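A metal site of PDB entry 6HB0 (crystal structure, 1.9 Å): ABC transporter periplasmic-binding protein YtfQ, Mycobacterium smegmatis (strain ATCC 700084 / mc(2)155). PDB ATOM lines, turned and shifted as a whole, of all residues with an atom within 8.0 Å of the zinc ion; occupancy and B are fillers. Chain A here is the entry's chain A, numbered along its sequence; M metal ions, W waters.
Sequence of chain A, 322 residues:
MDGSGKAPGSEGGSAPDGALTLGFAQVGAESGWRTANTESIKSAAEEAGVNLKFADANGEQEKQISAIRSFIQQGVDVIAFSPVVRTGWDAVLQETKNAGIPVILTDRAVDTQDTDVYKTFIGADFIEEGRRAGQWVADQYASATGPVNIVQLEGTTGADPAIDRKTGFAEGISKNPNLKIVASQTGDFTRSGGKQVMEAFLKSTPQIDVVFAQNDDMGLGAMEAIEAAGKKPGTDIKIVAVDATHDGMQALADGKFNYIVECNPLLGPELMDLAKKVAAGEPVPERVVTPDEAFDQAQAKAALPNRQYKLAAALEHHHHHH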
ATOM      1  N   GLY A 123     -18.249   8.693 -21.867  1.00  0.00           N
ATOM      2  CA  GLY A 123     -18.574   9.692 -22.907  1.00  0.00           C
ATOM      3  C   GLY A 123     -18.693  11.104 -22.376  1.00  0.00           C
ATOM      4  O   GLY A 123     -18.677  11.285 -21.185  1.00  0.00           O
ATOM      5  N   ALA A 124     -18.824  12.065 -23.283  1.00  0.00           N
ATOM      6  CA  ALA A 124     -18.867  13.467 -22.915  1.00  0.00           C
ATOM      7  C   ALA A 124     -20.213  13.807 -22.305  1.00  0.00           C
ATOM      8  O   ALA A 124     -21.200  13.125 -22.574  1.00  0.00           O
ATOM      9  CB  ALA A 124     -18.619  14.359 -24.108  1.00  0.00           C
ATOM     10  N   ASP A 125     -20.216  14.835 -21.465  1.00  0.00           N
ATOM     11  CA  ASP A 125     -21.398  15.371 -20.837  1.00  0.00           C
ATOM     12  C   ASP A 125     -21.793  16.759 -21.387  1.00  0.00           C
ATOM     13  O   ASP A 125     -21.227  17.806 -21.001  1.00  0.00           O
ATOM     14  CB  ASP A 125     -21.091  15.510 -19.364  1.00  0.00           C
ATOM     15  CG  ASP A 125     -22.332  15.791 -18.501  1.00  0.00           C
ATOM     16  OD1 ASP A 125     -23.389  16.227 -19.022  1.00  0.00           O
ATOM     17  OD2 ASP A 125     -22.221  15.601 -17.283  1.00  0.00           O
ATOM     18  N   PHE A 126     -22.790  16.797 -22.264  1.00  0.00           N
ATOM     19  CA  PHE A 126     -23.150  18.053 -22.900  1.00  0.00           C
ATOM     20  C   PHE A 126     -23.877  19.027 -21.974  1.00  0.00           C
ATOM     21  O   PHE A 126     -23.778  20.247 -22.156  1.00  0.00           O
ATOM     22  CB  PHE A 126     -24.033  17.781 -24.096  1.00  0.00           C
ATOM     23  CG  PHE A 126     -23.411  16.888 -25.124  1.00  0.00           C
ATOM     24  CD1 PHE A 126     -22.117  17.130 -25.591  1.00  0.00           C
ATOM     25  CD2 PHE A 126     -24.106  15.796 -25.616  1.00  0.00           C
ATOM     26  CE1 PHE A 126     -21.554  16.325 -26.547  1.00  0.00           C
ATOM     27  CE2 PHE A 126     -23.530  14.962 -26.553  1.00  0.00           C
ATOM     28  CZ  PHE A 126     -22.273  15.249 -27.031  1.00  0.00           C
ATOM     29  N   GLU A 128     -23.173  19.358 -18.818  1.00  0.00           N
ATOM     30  CA  GLU A 128     -22.040  19.937 -18.110  1.00  0.00           C
ATOM     31  C   GLU A 128     -21.376  21.044 -18.920  1.00  0.00           C
ATOM     32  O   GLU A 128     -21.011  22.072 -18.364  1.00  0.00           O
ATOM     33  CB  GLU A 128     -21.068  18.829 -17.733  1.00  0.00           C
ATOM     34  CG  GLU A 128     -19.754  19.259 -17.136  1.00  0.00           C
ATOM     35  CD  GLU A 128     -18.596  18.741 -17.982  1.00  0.00           C
ATOM     36  OE1 GLU A 128     -18.091  19.502 -18.845  1.00  0.00           O
ATOM     37  OE2 GLU A 128     -18.262  17.528 -17.838  1.00  0.00           O
ATOM     38  N   GLU A 129     -21.201  20.878 -20.225  1.00  0.00           N
ATOM     39  CA  GLU A 129     -20.671  21.946 -21.077  1.00  0.00           C
ATOM     40  C   GLU A 129     -21.467  23.238 -20.977  1.00  0.00           C
ATOM     41  O   GLU A 129     -20.909  24.304 -20.766  1.00  0.00           O
ATOM     42  CB  GLU A 129     -20.572  21.546 -22.570  1.00  0.00           C
ATOM     43  CG  GLU A 129     -19.473  20.492 -22.845  1.00  0.00           C
ATOM     44  CD  GLU A 129     -19.431  20.051 -24.315  1.00  0.00           C
ATOM     45  OE1 GLU A 129     -20.537  19.896 -24.922  1.00  0.00           O
ATOM     46  OE2 GLU A 129     -18.280  19.849 -24.841  1.00  0.00           O
ATOM     47  N   ARG A 132     -21.152  24.820 -17.511  1.00  0.00           N
ATOM     48  CA  ARG A 132     -19.880  25.557 -17.268  1.00  0.00           C
ATOM     49  C   ARG A 132     -19.894  26.892 -18.019  1.00  0.00           C
ATOM     50  O   ARG A 132     -19.344  27.902 -17.533  1.00  0.00           O
ATOM     51  CB  ARG A 132     -18.669  24.667 -17.629  1.00  0.00           C
ATOM     52  CG  ARG A 132     -18.554  23.440 -16.718  1.00  0.00           C
ATOM     53  CD  ARG A 132     -17.784  22.283 -17.336  1.00  0.00           C
ATOM     54  NE  ARG A 132     -16.520  22.781 -17.755  1.00  0.00           N
ATOM     55  CZ  ARG A 132     -15.825  22.377 -18.817  1.00  0.00           C
ATOM     56  NH1 ARG A 132     -16.154  21.346 -19.596  1.00  0.00           N
ATOM     57  NH2 ARG A 132     -14.712  23.046 -19.068  1.00  0.00           N
ATOM     58  N   GLU A 262     -15.105  22.852 -23.143  1.00  0.00           N
ATOM     59  CA  GLU A 262     -15.309  21.594 -23.870  1.00  0.00           C
ATOM     60  C   GLU A 262     -15.273  20.484 -22.899  1.00  0.00           C
ATOM     61  O   GLU A 262     -14.470  20.515 -21.977  1.00  0.00           O
ATOM     62  CB  GLU A 262     -14.242  21.378 -24.923  1.00  0.00           C
ATOM     63  CG  GLU A 262     -14.488  20.119 -25.740  1.00  0.00           C
ATOM     64  CD  GLU A 262     -13.446  19.838 -26.800  1.00  0.00           C
ATOM     65  OE1 GLU A 262     -13.089  20.791 -27.502  1.00  0.00           O
ATOM     66  OE2 GLU A 262     -13.028  18.644 -26.968  1.00  0.00           O
ATOM     67  N   CYS A 263     -16.164  19.506 -23.060  1.00  0.00           N
ATOM     68  CA  CYS A 263     -16.089  18.246 -22.388  1.00  0.00           C
ATOM     69  C   CYS A 263     -15.524  17.295 -23.450  1.00  0.00           C
ATOM     70  O   CYS A 263     -16.133  17.108 -24.513  1.00  0.00           O
ATOM     71  CB  CYS A 263     -17.443  17.742 -21.927  1.00  0.00           C
ATOM     72  SG  CYS A 263     -17.355  16.205 -20.978  1.00  0.00           S
ATOM     73  N   ASN A 264     -14.387  16.693 -23.183  1.00  0.00           N
ATOM     74  CA  ASN A 264     -13.757  15.819 -24.161  1.00  0.00           C
ATOM     75  C   ASN A 264     -14.539  14.509 -24.409  1.00  0.00           C
ATOM     76  O   ASN A 264     -15.241  13.992 -23.563  1.00  0.00           O
ATOM     77  CB  ASN A 264     -12.361  15.378 -23.708  1.00  0.00           C
ATOM     78  CG  ASN A 264     -11.332  16.457 -23.730  1.00  0.00           C
ATOM     79  OD1 ASN A 264     -10.340  16.327 -23.035  1.00  0.00           O
ATOM     80  ND2 ASN A 264     -11.501  17.478 -24.525  1.00  0.00           N
ATOM     81  N   PRO A 265     -14.371  13.971 -25.615  1.00  0.00           N
ATOM     82  CA  PRO A 265     -14.706  12.560 -25.750  1.00  0.00           C
ATOM     83  C   PRO A 265     -13.695  11.681 -25.018  1.00  0.00           C
ATOM     84  O   PRO A 265     -12.677  12.159 -24.441  1.00  0.00           O
ATOM     85  CB  PRO A 265     -14.604  12.323 -27.251  1.00  0.00           C
ATOM     86  CG  PRO A 265     -13.513  13.250 -27.661  1.00  0.00           C
ATOM     87  CD  PRO A 265     -13.668  14.485 -26.780  1.00  0.00           C
ATOM     88  N   ARG A 287     -20.149   4.519 -14.831  1.00  0.00           N
ATOM     89  CA  ARG A 287     -19.793   5.651 -15.660  1.00  0.00           C
ATOM     90  C   ARG A 287     -18.370   6.102 -15.327  1.00  0.00           C
ATOM     91  O   ARG A 287     -17.982   6.088 -14.157  1.00  0.00           O
ATOM     92  CB  ARG A 287     -20.778   6.794 -15.404  1.00  0.00           C
ATOM     93  CG  ARG A 287     -20.519   7.976 -16.295  1.00  0.00           C
ATOM     94  CD  ARG A 287     -21.651   8.970 -16.325  1.00  0.00           C
ATOM     95  NE  ARG A 287     -21.070  10.231 -16.832  1.00  0.00           N
ATOM     96  CZ  ARG A 287     -21.202  11.448 -16.294  1.00  0.00           C
ATOM     97  NH1 ARG A 287     -22.001  11.644 -15.241  1.00  0.00           N
ATOM     98  NH2 ARG A 287     -20.579  12.504 -16.855  1.00  0.00           N
ATOM     99  N   VAL A 289     -15.854   9.401 -16.257  1.00  0.00           N
ATOM    100  CA  VAL A 289     -15.933  10.726 -16.826  1.00  0.00           C
ATOM    101  C   VAL A 289     -14.788  11.050 -17.726  1.00  0.00           C
ATOM    102  O   VAL A 289     -13.722  10.534 -17.557  1.00  0.00           O
ATOM    103  CB  VAL A 289     -15.878  11.851 -15.745  1.00  0.00           C
ATOM    104  CG1 VAL A 289     -17.081  11.712 -14.861  1.00  0.00           C
ATOM    105  CG2 VAL A 289     -14.559  11.826 -14.949  1.00  0.00           C
ATOM    106  N   THR A 290     -15.039  11.866 -18.723  1.00  0.00           N
ATOM    107  CA  THR A 290     -13.979  12.278 -19.613  1.00  0.00           C
ATOM    108  C   THR A 290     -13.365  13.555 -19.036  1.00  0.00           C
ATOM    109  O   THR A 290     -13.993  14.238 -18.265  1.00  0.00           O
ATOM    110  CB  THR A 290     -14.500  12.528 -21.026  1.00  0.00           C
ATOM    111  OG1 THR A 290     -15.589  13.464 -20.977  1.00  0.00           O
ATOM    112  CG2 THR A 290     -14.972  11.235 -21.658  1.00  0.00           C
ATOM    113  N   PRO A 291     -12.146  13.884 -19.459  1.00  0.00           N
ATOM    114  CA  PRO A 291     -11.597  15.173 -19.082  1.00  0.00           C
ATOM    115  C   PRO A 291     -12.247  16.397 -19.748  1.00  0.00           C
ATOM    116  O   PRO A 291     -12.901  16.283 -20.784  1.00  0.00           O
ATOM    117  CB  PRO A 291     -10.120  15.077 -19.535  1.00  0.00           C
ATOM    118  CG  PRO A 291      -9.961  13.801 -20.219  1.00  0.00           C
ATOM    119  CD  PRO A 291     -11.272  13.134 -20.365  1.00  0.00           C
ATOM    120  N   ASP A 292     -11.987  17.559 -19.164  1.00  0.00           N
ATOM    121  CA  ASP A 292     -12.472  18.817 -19.628  1.00  0.00           C
ATOM    122  C   ASP A 292     -11.392  19.764 -20.042  1.00  0.00           C
ATOM    123  O   ASP A 292     -10.240  19.642 -19.621  1.00  0.00           O
ATOM    124  CB  ASP A 292     -13.278  19.464 -18.483  1.00  0.00           C
ATOM    125  CG  ASP A 292     -14.560  18.715 -18.166  1.00  0.00           C
ATOM    126  OD1 ASP A 292     -15.122  18.061 -19.075  1.00  0.00           O
ATOM    127  OD2 ASP A 292     -15.027  18.804 -17.006  1.00  0.00           O
ATOM    128  N   GLU A 293     -11.764  20.745 -20.874  1.00  0.00           N
ATOM    129  CA  GLU A 293     -10.922  21.855 -21.250  1.00  0.00           C
ATOM    130  C   GLU A 293     -11.701  23.133 -21.032  1.00  0.00           C
ATOM    131  O   GLU A 293     -12.961  23.160 -21.137  1.00  0.00           O
ATOM    132  CB  GLU A 293     -10.501  21.795 -22.710  1.00  0.00           C
ATOM    133  CG  GLU A 293      -9.698  20.547 -23.036  1.00  0.00           C
ATOM    134  CD  GLU A 293      -9.283  20.427 -24.512  1.00  0.00           C
ATOM    135  OE1 GLU A 293      -8.777  21.405 -25.068  1.00  0.00           O
ATOM    136  OE2 GLU A 293      -9.377  19.318 -25.064  1.00  0.00           O
HETATM  137 ZN    ZN M   1     -16.711  16.993 -18.948  1.00  0.00          ZN
HETATM  138  O   HOH W   1     -16.271  15.406 -17.771  1.00  0.00           O
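The zinc ion is bound by OD1 of Asp 292, OE2 of Glu 128, water W1 and SG of Cys 263.
The zinc ion has four donor atoms within binding distance.
Thr 290 touches the zinc ion.
The nearest printed residue that does not touch the zinc ion is Pro 291 (4.3 Å).
OG1 of Thr 290 is in hydrogen-bond range of O of Asn 264 (2.7 Å).
The side-chain hydroxyl (OG1) of Thr 290 lies close to the side-chain sulfur (SG) of Cys 263.
The side-chain carboxylate of Asp 292 is in salt-bridge range of the guanidinium group of Arg 132 (3.8 Å).
The backbone NH (N) of Cys 263 sits at hydrogen-bond distance from the side-chain carboxylate (OE2) of Glu 129 (2.8 Å).
SG of Cys 263 lies close to N of Asp 125.
The guanidinium group (NH1) of Arg 132 is in salt-bridge range of the side-chain carboxylate (OE1) of Glu 128, 2.8 Å away.
N of Glu 128 is in hydrogen-bond range of OD1 of Asp 125.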
